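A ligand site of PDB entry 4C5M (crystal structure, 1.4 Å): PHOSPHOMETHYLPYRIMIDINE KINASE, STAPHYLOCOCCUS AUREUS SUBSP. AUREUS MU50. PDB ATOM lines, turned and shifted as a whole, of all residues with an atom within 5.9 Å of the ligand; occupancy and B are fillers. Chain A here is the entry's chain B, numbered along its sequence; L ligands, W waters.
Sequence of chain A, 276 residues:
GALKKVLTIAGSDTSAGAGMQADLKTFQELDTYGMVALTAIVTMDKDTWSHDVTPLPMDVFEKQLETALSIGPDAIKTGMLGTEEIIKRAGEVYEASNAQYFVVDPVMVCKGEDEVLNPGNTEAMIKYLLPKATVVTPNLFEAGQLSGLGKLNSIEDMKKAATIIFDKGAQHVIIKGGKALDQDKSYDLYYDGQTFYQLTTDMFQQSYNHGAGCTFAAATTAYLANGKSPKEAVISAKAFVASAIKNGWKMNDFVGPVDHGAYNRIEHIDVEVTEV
An oxygen (O7) of the ligand is in salt-bridge range of the side-chain amino group (NZ) of Lys 176.
An oxygen (O12) of the ligand lies within hydrogen-bond range of the side-chain carboxylate (OD1) of Asp 188 (2.7 Å).
O12 of the ligand is in hydrogen-bond range of OG of Ser 186 (2.7 Å).
N of Gly 211 sits at hydrogen-bond distance from O1 of the ligand, at 2.7 Å.
The backbone NH (N) of Gly 213 sits close to an oxygen (O8) of the ligand.
N of Phe 204 lies within hydrogen-bond range of N4 of the ligand (3.0 Å).
The backbone carbonyl oxygen of Phe 204 is in hydrogen-bond range of a nitrogen (N3) of the ligand.
The backbone NH of Cys 214 sits at hydrogen-bond distance from an oxygen (O2) of the ligand (3.0 Å).
The side-chain sulfur (SG) of Cys 214 sits at hydrogen-bond distance from an oxygen (O2) of the ligand, 3.4 Å away.
The side-chain amino group (NZ) of Lys 238 is in hydrogen-bond range of an oxygen (O12) of the ligand (3.1 Å).
N3 of the ligand sits at hydrogen-bond distance from OD1 of Asn 209 (3.2 Å).
The side-chain sulfur (SD) of Met 203 lies close to a nitrogen (N3) of the ligand, 3.5 Å away.
The side-chain amino group (NZ) of Lys 179 lies within salt-bridge range of an oxygen (O5) of the ligand.
A nitrogen (N3) of the ligand sits at hydrogen-bond distance from the backbone carbonyl oxygen of Gln 205 (3.4 Å).
The backbone carbonyl oxygen of Pro 138 sits at hydrogen-bond distance from the backbone NH of Lys 176.
The backbone carbonyl oxygen of Thr 137 sits close to the side-chain amino group of Lys 176 (3.1 Å).
The side-chain carboxylate (OD1) of Asp 188 sits at hydrogen-bond distance from the backbone NH (N) of Gly 177, at 3.1 Å.
The backbone carbonyl oxygen of Ser 186 sits at hydrogen-bond distance from the side-chain amino group of Lys 238 (3.1 Å).
The backbone NH of Gly 19 sits at hydrogen-bond distance from the side-chain sulfur of Cys 214 (3.4 Å).
The side-chain amide nitrogen of Asn 209 lies within hydrogen-bond range of the backbone carbonyl oxygen of Gln 205, at 2.9 Å.
SD of Met 203 lies close to OE1 of Gln 206, at 3.7 Å.
The backbone NH of Gly 178 lies within hydrogen-bond range of the backbone carbonyl oxygen of Tyr 187 (3.0 Å).
Ala 18 touches the ligand.
Asn 139 touches the ligand.
CA of Gly 178 touches O12 of the ligand, 3.7 Å away.
O of Asp 202 touches C10 of the ligand (3.6 Å).
Gln 206 touches the ligand (CG to N3, 3.8 Å).
His 210 touches the ligand (ND1 to O1, 3.6 Å).
Ala 212 touches the ligand.
Phe 216 touches the ligand.
Val 241 touches the ligand.
Ile 245 touches the ligand.
Hydrophobic or aromatic side chains that line the ligand: Ala 18, Met 203, Phe 204, Ala 212, Phe 216, Val 241 and Ile 245.
Within 4 Å of the ligand: Ala 18, Asn 139, Lys 176, Gly 178, Lys 179, Ser 186, Asp 188, Asp 202, Met 203, Phe 204, Gln 205, Gln 206, Asn 209, His 210, Gly 211, Ala 212, Gly 213, Cys 214, Phe 216, Lys 238, Val 241 and Ile 245.
Water W4 lies within hydrogen-bond range of an oxygen (O4) of the ligand (2.6 Å) and the side-chain amide nitrogen (ND2) of Asn 139 (3.1 Å).
Water W5 lies within hydrogen-bond range of the backbone NH of Lys 179, an oxygen (O6) of the ligand and the backbone carbonyl oxygen of Gly 177.
Water W3 bridges an oxygen (O3) of the ligand (2.9 Å) and the side-chain sulfur (SG) of Cys 214 (3.6 Å).
Water W2 lies within hydrogen-bond range of the side-chain amino group (NZ) of Lys 238 (2.7 Å), the side-chain hydroxyl (OG1) of Thr 201 (2.8 Å) and a nitrogen (N5) of the ligand (3.0 Å).
Water W1 bridges ND1 of His 210 (2.7 Å) and O1 of the ligand (3.2 Å).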
ATOM      1  N   GLY A  17      -3.526  -2.464  -9.717  1.00  0.00           N
ATOM      2  CA  GLY A  17      -4.230  -3.487  -9.014  1.00  0.00           C
ATOM      3  C   GLY A  17      -5.290  -4.184  -9.812  1.00  0.00           C
ATOM      4  O   GLY A  17      -5.590  -5.328  -9.513  1.00  0.00           O
ATOM      5  N   ALA A  18      -5.835  -3.484 -10.806  1.00  0.00           N
ATOM      6  CA  ALA A  18      -6.884  -3.965 -11.677  1.00  0.00           C
ATOM      7  C   ALA A  18      -6.436  -3.833 -13.123  1.00  0.00           C
ATOM      8  O   ALA A  18      -5.232  -3.725 -13.416  1.00  0.00           O
ATOM      9  CB  ALA A  18      -8.177  -3.210 -11.396  1.00  0.00           C
ATOM     10  N   GLY A  19      -7.369  -3.852 -14.047  1.00  0.00           N
ATOM     11  CA  GLY A  19      -7.055  -3.681 -15.464  1.00  0.00           C
ATOM     12  C   GLY A  19      -6.082  -4.725 -15.975  1.00  0.00           C
ATOM     13  O   GLY A  19      -5.961  -5.840 -15.446  1.00  0.00           O
ATOM     14  N   THR A 137     -18.623 -13.328 -16.785  1.00  0.00           N
ATOM     15  CA  THR A 137     -18.359 -13.159 -15.345  1.00  0.00           C
ATOM     16  C   THR A 137     -18.918 -11.854 -14.798  1.00  0.00           C
ATOM     17  O   THR A 137     -18.193 -11.099 -14.213  1.00  0.00           O
ATOM     18  CB  THR A 137     -16.827 -13.256 -15.091  1.00  0.00           C
ATOM     19  OG1 THR A 137     -16.177 -12.180 -15.738  1.00  0.00           O
ATOM     20  CG2 THR A 137     -16.225 -14.522 -15.613  1.00  0.00           C
ATOM     21  N   PRO A 138     -20.242 -11.619 -14.885  1.00  0.00           N
ATOM     22  CA  PRO A 138     -20.789 -10.367 -14.292  1.00  0.00           C
ATOM     23  C   PRO A 138     -20.773 -10.344 -12.764  1.00  0.00           C
ATOM     24  O   PRO A 138     -21.031 -11.379 -12.123  1.00  0.00           O
ATOM     25  CB  PRO A 138     -22.263 -10.387 -14.763  1.00  0.00           C
ATOM     26  CG  PRO A 138     -22.570 -11.853 -14.932  1.00  0.00           C
ATOM     27  CD  PRO A 138     -21.309 -12.443 -15.489  1.00  0.00           C
ATOM     28  N   ASN A 139     -20.539  -9.181 -12.206  1.00  0.00           N
ATOM     29  CA  ASN A 139     -20.875  -8.935 -10.832  1.00  0.00           C
ATOM     30  C   ASN A 139     -22.380  -8.756 -10.705  1.00  0.00           C
ATOM     31  O   ASN A 139     -23.126  -8.825 -11.696  1.00  0.00           O
ATOM     32  CB  ASN A 139     -20.046  -7.810 -10.243  1.00  0.00           C
ATOM     33  CG  ASN A 139     -20.356  -6.448 -10.825  1.00  0.00           C
ATOM     34  OD1 ASN A 139     -21.480  -6.146 -11.303  1.00  0.00           O
ATOM     35  ND2 ASN A 139     -19.363  -5.572 -10.730  1.00  0.00           N
ATOM     36  N   LYS A 176     -21.261 -13.097  -9.664  1.00  0.00           N
ATOM     37  CA  LYS A 176     -20.616 -12.910  -8.384  1.00  0.00           C
ATOM     38  C   LYS A 176     -21.509 -12.098  -7.437  1.00  0.00           C
ATOM     39  O   LYS A 176     -22.009 -11.029  -7.809  1.00  0.00           O
ATOM     40  CB  LYS A 176     -19.268 -12.212  -8.606  1.00  0.00           C
ATOM     41  CG  LYS A 176     -18.349 -13.049  -9.480  1.00  0.00           C
ATOM     42  CD  LYS A 176     -17.218 -12.226 -10.088  1.00  0.00           C
ATOM     43  CE  LYS A 176     -17.796 -11.370 -11.188  1.00  0.00           C
ATOM     44  NZ  LYS A 176     -16.906 -10.247 -11.498  1.00  0.00           N
ATOM     45  N   GLY A 177     -21.769 -12.625  -6.263  1.00  0.00           N
ATOM     46  CA  GLY A 177     -22.568 -11.921  -5.262  1.00  0.00           C
ATOM     47  C   GLY A 177     -21.625 -11.142  -4.424  1.00  0.00           C
ATOM     48  O   GLY A 177     -21.596  -9.912  -4.459  1.00  0.00           O
ATOM     49  N   GLY A 178     -20.870 -11.863  -3.621  1.00  0.00           N
ATOM     50  CA  GLY A 178     -19.848 -11.257  -2.817  1.00  0.00           C
ATOM     51  C   GLY A 178     -20.412 -10.282  -1.813  1.00  0.00           C
ATOM     52  O   GLY A 178     -21.469 -10.548  -1.174  1.00  0.00           O
ATOM     53  N   LYS A 179     -19.729  -9.140  -1.674  1.00  0.00           N
ATOM     54  CA  LYS A 179     -20.090  -8.111  -0.669  1.00  0.00           C
ATOM     55  C   LYS A 179     -21.426  -7.515  -0.969  1.00  0.00           C
ATOM     56  O   LYS A 179     -22.069  -7.017  -0.079  1.00  0.00           O
ATOM     57  CB  LYS A 179     -19.123  -6.914  -0.680  1.00  0.00           C
ATOM     58  CG  LYS A 179     -17.683  -7.213  -0.446  1.00  0.00           C
ATOM     59  CD  LYS A 179     -16.881  -5.915  -0.290  1.00  0.00           C
ATOM     60  CE  LYS A 179     -16.562  -5.203  -1.598  1.00  0.00           C
ATOM     61  NZ  LYS A 179     -15.619  -5.991  -2.439  1.00  0.00           N
ATOM     62  N   SER A 186     -19.318 -15.203   1.275  1.00  0.00           N
ATOM     63  CA  SER A 186     -19.241 -14.690  -0.059  1.00  0.00           C
ATOM     64  C   SER A 186     -19.771 -15.719  -1.052  1.00  0.00           C
ATOM     65  O   SER A 186     -19.089 -16.711  -1.345  1.00  0.00           O
ATOM     66  CB  SER A 186     -17.803 -14.362  -0.411  1.00  0.00           C
ATOM     67  OG  SER A 186     -17.771 -13.822  -1.707  1.00  0.00           O
ATOM     68  N   TYR A 187     -20.953 -15.418  -1.586  1.00  0.00           N
ATOM     69  CA  TYR A 187     -21.665 -16.304  -2.515  1.00  0.00           C
ATOM     70  C   TYR A 187     -21.563 -15.858  -3.942  1.00  0.00           C
ATOM     71  O   TYR A 187     -21.801 -14.686  -4.232  1.00  0.00           O
ATOM     72  CB  TYR A 187     -23.150 -16.401  -2.173  1.00  0.00           C
ATOM     73  CG  TYR A 187     -23.506 -16.818  -0.771  1.00  0.00           C
ATOM     74  CD1 TYR A 187     -23.602 -18.141  -0.440  1.00  0.00           C
ATOM     75  CD2 TYR A 187     -23.773 -15.885   0.221  1.00  0.00           C
ATOM     76  CE1 TYR A 187     -23.950 -18.554   0.848  1.00  0.00           C
ATOM     77  CE2 TYR A 187     -24.118 -16.284   1.525  1.00  0.00           C
ATOM     78  CZ  TYR A 187     -24.202 -17.617   1.822  1.00  0.00           C
ATOM     79  OH  TYR A 187     -24.509 -18.011   3.114  1.00  0.00           O
ATOM     80  N   ASP A 188     -21.224 -16.785  -4.831  1.00  0.00           N
ATOM     81  CA  ASP A 188     -21.355 -16.624  -6.262  1.00  0.00           C
ATOM     82  C   ASP A 188     -22.247 -17.739  -6.809  1.00  0.00           C
ATOM     83  O   ASP A 188     -22.379 -18.787  -6.178  1.00  0.00           O
ATOM     84  CB  ASP A 188     -19.995 -16.664  -6.988  1.00  0.00           C
ATOM     85  CG  ASP A 188     -18.975 -15.701  -6.407  1.00  0.00           C
ATOM     86  OD1 ASP A 188     -19.350 -14.582  -6.007  1.00  0.00           O
ATOM     87  OD2 ASP A 188     -17.780 -16.080  -6.400  1.00  0.00           O
ATOM     88  N   THR A 201     -17.154 -18.956  -0.092  1.00  0.00           N
ATOM     89  CA  THR A 201     -16.069 -18.887   0.870  1.00  0.00           C
ATOM     90  C   THR A 201     -16.539 -17.991   2.011  1.00  0.00           C
ATOM     91  O   THR A 201     -17.592 -17.353   1.938  1.00  0.00           O
ATOM     92  CB  THR A 201     -14.738 -18.303   0.321  1.00  0.00           C
ATOM     93  OG1 THR A 201     -14.880 -16.903   0.081  1.00  0.00           O
ATOM     94  CG2 THR A 201     -14.253 -19.005  -0.955  1.00  0.00           C
ATOM     95  N   ASP A 202     -15.722 -17.883   3.049  1.00  0.00           N
ATOM     96  CA  ASP A 202     -15.952 -16.882   4.057  1.00  0.00           C
ATOM     97  C   ASP A 202     -15.857 -15.513   3.388  1.00  0.00           C
ATOM     98  O   ASP A 202     -15.239 -15.339   2.322  1.00  0.00           O
ATOM     99  CB  ASP A 202     -14.925 -16.987   5.197  1.00  0.00           C
ATOM    100  CG  ASP A 202     -15.097 -18.246   6.051  1.00  0.00           C
ATOM    101  OD1 ASP A 202     -16.164 -18.920   5.989  1.00  0.00           O
ATOM    102  OD2 ASP A 202     -14.146 -18.559   6.795  1.00  0.00           O
ATOM    103  N   MET A 203     -16.512 -14.556   4.004  1.00  0.00           N
ATOM    104  CA  MET A 203     -16.318 -13.158   3.685  1.00  0.00           C
ATOM    105  C   MET A 203     -15.059 -12.697   4.365  1.00  0.00           C
ATOM    106  O   MET A 203     -14.920 -12.865   5.571  1.00  0.00           O
ATOM    107  CB  MET A 203     -17.503 -12.298   4.205  1.00  0.00           C
ATOM    108  CG  MET A 203     -17.472 -10.819   3.732  1.00  0.00           C
ATOM    109  SD  MET A 203     -17.565 -10.512   1.935  1.00  0.00           S
ATOM    110  CE  MET A 203     -18.879 -11.710   1.733  1.00  0.00           C
ATOM    111  N   PHE A 204     -14.162 -12.116   3.592  1.00  0.00           N
ATOM    112  CA  PHE A 204     -12.952 -11.535   4.131  1.00  0.00           C
ATOM    113  C   PHE A 204     -13.060 -10.013   4.169  1.00  0.00           C
ATOM    114  O   PHE A 204     -14.061  -9.423   3.752  1.00  0.00           O
ATOM    115  CB  PHE A 204     -11.756 -12.028   3.296  1.00  0.00           C
ATOM    116  CG  PHE A 204     -11.648 -13.528   3.266  1.00  0.00           C
ATOM    117  CD1 PHE A 204     -11.274 -14.198   4.409  1.00  0.00           C
ATOM    118  CD2 PHE A 204     -11.960 -14.274   2.119  1.00  0.00           C
ATOM    119  CE1 PHE A 204     -11.180 -15.590   4.420  1.00  0.00           C
ATOM    120  CE2 PHE A 204     -11.854 -15.672   2.133  1.00  0.00           C
ATOM    121  CZ  PHE A 204     -11.461 -16.312   3.287  1.00  0.00           C
ATOM    122  N   GLN A 205     -12.006  -9.396   4.661  1.00  0.00           N
ATOM    123  CA  GLN A 205     -11.975  -7.961   4.808  1.00  0.00           C
ATOM    124  C   GLN A 205     -12.355  -7.250   3.521  1.00  0.00           C
ATOM    125  O   GLN A 205     -12.041  -7.697   2.437  1.00  0.00           O
ATOM    126  CB  GLN A 205     -10.591  -7.518   5.293  1.00  0.00           C
ATOM    127  CG  GLN A 205      -9.439  -7.747   4.338  1.00  0.00           C
ATOM    128  CD  GLN A 205      -9.293  -6.705   3.250  1.00  0.00           C
ATOM    129  OE1 GLN A 205      -9.633  -5.533   3.435  1.00  0.00           O
ATOM    130  NE2 GLN A 205      -8.729  -7.123   2.100  1.00  0.00           N
ATOM    131  N   GLN A 206     -13.085  -6.150   3.672  1.00  0.00           N
ATOM    132  CA  GLN A 206     -13.717  -5.470   2.548  1.00  0.00           C
ATOM    133  C   GLN A 206     -13.040  -4.163   2.217  1.00  0.00           C
ATOM    134  O   GLN A 206     -13.436  -3.535   1.263  1.00  0.00           O
ATOM    135  CB  GLN A 206     -15.222  -5.226   2.820  1.00  0.00           C
ATOM    136  CG  GLN A 206     -15.976  -6.507   3.153  1.00  0.00           C
ATOM    137  CD  GLN A 206     -17.493  -6.356   3.334  1.00  0.00           C
ATOM    138  OE1 GLN A 206     -18.199  -7.321   3.634  1.00  0.00           O
ATOM    139  NE2 GLN A 206     -18.002  -5.182   3.127  1.00  0.00           N
ATOM    140  N   ASN A 209      -9.923  -4.371  -1.561  1.00  0.00           N
ATOM    141  CA  ASN A 209     -10.393  -5.368  -2.512  1.00  0.00           C
ATOM    142  C   ASN A 209     -10.211  -4.867  -3.960  1.00  0.00           C
ATOM    143  O   ASN A 209     -10.835  -5.421  -4.890  1.00  0.00           O
ATOM    144  CB  ASN A 209     -11.909  -5.626  -2.318  1.00  0.00           C
ATOM    145  CG  ASN A 209     -12.313  -6.307  -0.997  1.00  0.00           C
ATOM    146  OD1 ASN A 209     -13.507  -6.485  -0.778  1.00  0.00           O
ATOM    147  ND2 ASN A 209     -11.376  -6.674  -0.149  1.00  0.00           N
ATOM    148  N   HIS A 210      -9.317  -3.894  -4.191  1.00  0.00           N
ATOM    149  CA  HIS A 210      -9.158  -3.363  -5.526  1.00  0.00           C
ATOM    150  C   HIS A 210      -8.532  -4.402  -6.457  1.00  0.00           C
ATOM    151  O   HIS A 210      -7.510  -4.968  -6.133  1.00  0.00           O
ATOM    152  CB  HIS A 210      -8.326  -2.090  -5.529  1.00  0.00           C
ATOM    153  CG  HIS A 210      -8.155  -1.504  -6.902  1.00  0.00           C
ATOM    154  ND1 HIS A 210      -9.208  -1.003  -7.648  1.00  0.00           N
ATOM    155  CD2 HIS A 210      -7.040  -1.278  -7.649  1.00  0.00           C
ATOM    156  CE1 HIS A 210      -8.752  -0.561  -8.805  1.00  0.00           C
ATOM    157  NE2 HIS A 210      -7.441  -0.674  -8.810  1.00  0.00           N
ATOM    158  N   GLY A 211      -9.184  -4.631  -7.604  1.00  0.00           N
ATOM    159  CA  GLY A 211      -8.705  -5.619  -8.583  1.00  0.00           C
ATOM    160  C   GLY A 211      -9.314  -7.010  -8.418  1.00  0.00           C
ATOM    161  O   GLY A 211      -9.011  -7.878  -9.218  1.00  0.00           O
ATOM    162  N   ALA A 212     -10.207  -7.195  -7.432  1.00  0.00           N
ATOM    163  CA  ALA A 212     -10.788  -8.541  -7.258  1.00  0.00           C
ATOM    164  C   ALA A 212     -11.505  -9.046  -8.512  1.00  0.00           C
ATOM    165  O   ALA A 212     -11.376 -10.203  -8.906  1.00  0.00           O
ATOM    166  CB  ALA A 212     -11.746  -8.558  -6.087  1.00  0.00           C
ATOM    167  N   GLY A 213     -12.352  -8.199  -9.102  1.00  0.00           N
ATOM    168  CA  GLY A 213     -13.125  -8.590 -10.273  1.00  0.00           C
ATOM    169  C   GLY A 213     -12.227  -8.945 -11.440  1.00  0.00           C
ATOM    170  O   GLY A 213     -12.406  -9.984 -12.103  1.00  0.00           O
ATOM    171  N   CYS A 214     -11.259  -8.079 -11.722  1.00  0.00           N
ATOM    172  CA  CYS A 214     -10.375  -8.346 -12.857  1.00  0.00           C
ATOM    173  C   CYS A 214      -9.601  -9.630 -12.662  1.00  0.00           C
ATOM    174  O   CYS A 214      -9.458 -10.465 -13.560  1.00  0.00           O
ATOM    175  CB  CYS A 214      -9.442  -7.163 -13.132  1.00  0.00           C
ATOM    176  SG  CYS A 214     -10.249  -5.687 -13.735  1.00  0.00           S
ATOM    177  N   THR A 215      -9.119  -9.794 -11.434  1.00  0.00           N
ATOM    178  CA  THR A 215      -8.342 -10.962 -11.100  1.00  0.00           C
ATOM    179  C   THR A 215      -9.152 -12.238 -11.274  1.00  0.00           C
ATOM    180  O   THR A 215      -8.661 -13.266 -11.734  1.00  0.00           O
ATOM    181  CB  THR A 215      -7.797 -10.807  -9.680  1.00  0.00           C
ATOM    182  OG1 THR A 215      -6.985  -9.642  -9.624  1.00  0.00           O
ATOM    183  CG2 THR A 215      -6.928 -12.008  -9.265  1.00  0.00           C
ATOM    184  N   PHE A 216     -10.400 -12.193 -10.841  1.00  0.00           N
ATOM    185  CA  PHE A 216     -11.285 -13.344 -10.993  1.00  0.00           C
ATOM    186  C   PHE A 216     -11.387 -13.791 -12.453  1.00  0.00           C
ATOM    187  O   PHE A 216     -11.241 -14.988 -12.773  1.00  0.00           O
ATOM    188  CB  PHE A 216     -12.713 -13.076 -10.417  1.00  0.00           C
ATOM    189  CG  PHE A 216     -13.603 -14.243 -10.554  1.00  0.00           C
ATOM    190  CD1 PHE A 216     -13.668 -15.221  -9.591  1.00  0.00           C
ATOM    191  CD2 PHE A 216     -14.328 -14.382 -11.689  1.00  0.00           C
ATOM    192  CE1 PHE A 216     -14.449 -16.313  -9.786  1.00  0.00           C
ATOM    193  CE2 PHE A 216     -15.132 -15.455 -11.883  1.00  0.00           C
ATOM    194  CZ  PHE A 216     -15.172 -16.442 -10.943  1.00  0.00           C
ATOM    195  N   LYS A 238     -12.296 -18.548  -7.970  1.00  0.00           N
ATOM    196  CA  LYS A 238     -12.848 -17.976  -6.770  1.00  0.00           C
ATOM    197  C   LYS A 238     -11.873 -18.216  -5.622  1.00  0.00           C
ATOM    198  O   LYS A 238     -11.643 -17.333  -4.828  1.00  0.00           O
ATOM    199  CB  LYS A 238     -14.194 -18.568  -6.454  1.00  0.00           C
ATOM    200  CG  LYS A 238     -14.829 -17.992  -5.177  1.00  0.00           C
ATOM    201  CD  LYS A 238     -16.266 -18.484  -4.976  1.00  0.00           C
ATOM    202  CE  LYS A 238     -16.919 -17.948  -3.674  1.00  0.00           C
ATOM    203  NZ  LYS A 238     -17.007 -16.482  -3.630  1.00  0.00           N
ATOM    204  N   VAL A 241      -8.838 -15.805  -6.081  1.00  0.00           N
ATOM    205  CA  VAL A 241      -9.129 -14.427  -5.737  1.00  0.00           C
ATOM    206  C   VAL A 241      -9.456 -14.278  -4.237  1.00  0.00           C
ATOM    207  O   VAL A 241      -9.143 -13.233  -3.614  1.00  0.00           O
ATOM    208  CB  VAL A 241     -10.193 -13.779  -6.694  1.00  0.00           C
ATOM    209  CG1 VAL A 241     -11.589 -14.242  -6.377  1.00  0.00           C
ATOM    210  CG2 VAL A 241     -10.126 -12.267  -6.635  1.00  0.00           C
ATOM    211  N   ALA A 242     -10.063 -15.302  -3.630  1.00  0.00           N
ATOM    212  CA  ALA A 242     -10.345 -15.207  -2.185  1.00  0.00           C
ATOM    213  C   ALA A 242      -9.038 -15.011  -1.372  1.00  0.00           C
ATOM    214  O   ALA A 242      -8.991 -14.225  -0.460  1.00  0.00           O
ATOM    215  CB  ALA A 242     -11.117 -16.405  -1.693  1.00  0.00           C
ATOM    216  N   ILE A 245      -7.843 -11.480  -1.866  1.00  0.00           N
ATOM    217  CA  ILE A 245      -8.644 -10.542  -1.074  1.00  0.00           C
ATOM    218  C   ILE A 245      -8.281 -10.595   0.412  1.00  0.00           C
ATOM    219  O   ILE A 245      -8.054  -9.569   1.053  1.00  0.00           O
ATOM    220  CB  ILE A 245     -10.149 -10.856  -1.263  1.00  0.00           C
ATOM    221  CG1 ILE A 245     -10.611 -10.482  -2.641  1.00  0.00           C
ATOM    222  CG2 ILE A 245     -11.024 -10.170  -0.248  1.00  0.00           C
ATOM    223  CD1 ILE A 245     -11.976 -11.065  -2.992  1.00  0.00           C
HETATM  224  P1  LIG L   1     -12.328  -4.617  -9.504  1.00  0.00           P
HETATM  225  O1  LIG L   1     -11.484  -3.545  -8.641  1.00  0.00           O
HETATM  226  O2  LIG L   1     -11.345  -5.343 -10.570  1.00  0.00           O
HETATM  227  O3  LIG L   1     -13.425  -3.930 -10.235  1.00  0.00           O
HETATM  228  P2  LIG L   1     -14.659  -6.332  -7.488  1.00  0.00           P
HETATM  229  O4  LIG L   1     -15.653  -5.571  -8.260  1.00  0.00           O
HETATM  230  O5  LIG L   1     -14.842  -6.035  -5.927  1.00  0.00           O
HETATM  231  C1  LIG L   1     -12.973  -5.669  -8.044  1.00  0.00           C
HETATM  232  P3  LIG L   1     -16.410  -8.770  -7.687  1.00  0.00           P
HETATM  233  O6  LIG L   1     -17.449  -8.095  -6.837  1.00  0.00           O
HETATM  234  O7  LIG L   1     -16.697  -9.054  -9.155  1.00  0.00           O
HETATM  235  O8  LIG L   1     -14.955  -7.963  -7.631  1.00  0.00           O
HETATM  236  O9  LIG L   1     -16.181 -10.230  -7.003  1.00  0.00           O
HETATM  237  C2  LIG L   1     -14.939 -10.846  -7.386  1.00  0.00           C
HETATM  238  C3  LIG L   1     -14.789 -12.094  -6.541  1.00  0.00           C
HETATM  239  O10 LIG L   1     -14.427 -11.742  -5.173  1.00  0.00           O
HETATM  240  C4  LIG L   1     -16.030 -12.972  -6.406  1.00  0.00           C
HETATM  241  O11 LIG L   1     -15.623 -14.344  -6.356  1.00  0.00           O
HETATM  242  C5  LIG L   1     -16.648 -12.525  -5.098  1.00  0.00           C
HETATM  243  O12 LIG L   1     -17.428 -13.498  -4.413  1.00  0.00           O
HETATM  244  C6  LIG L   1     -15.458 -12.274  -4.261  1.00  0.00           C
HETATM  245  N1  LIG L   1     -15.449 -11.302  -3.172  1.00  0.00           N
HETATM  246  C7  LIG L   1     -15.578  -9.969  -3.367  1.00  0.00           C
HETATM  247  N2  LIG L   1     -15.359  -9.343  -2.206  1.00  0.00           N
HETATM  248  C8  LIG L   1     -15.090 -10.272  -1.261  1.00  0.00           C
HETATM  249  C9  LIG L   1     -14.738 -10.254   0.151  1.00  0.00           C
HETATM  250  N3  LIG L   1     -14.646  -9.085   0.767  1.00  0.00           N
HETATM  251  N4  LIG L   1     -14.537 -11.464   0.724  1.00  0.00           N
HETATM  252  C10 LIG L   1     -14.587 -12.629   0.043  1.00  0.00           C
HETATM  253  N5  LIG L   1     -14.903 -12.732  -1.258  1.00  0.00           N
HETATM  254  C11 LIG L   1     -15.133 -11.581  -1.922  1.00  0.00           C
HETATM  255  O   HOH W   1     -11.793  -0.896  -6.931  1.00  0.00           O
HETATM  256  O   HOH W   2     -14.766 -15.566  -2.357  1.00  0.00           O
HETATM  257  O   HOH W   3     -13.479  -4.200 -13.157  1.00  0.00           O
HETATM  258  O   HOH W   4     -16.450  -6.655 -10.470  1.00  0.00           O
HETATM  259  O   HOH W   5     -18.514  -8.670  -4.207  1.00  0.00           O
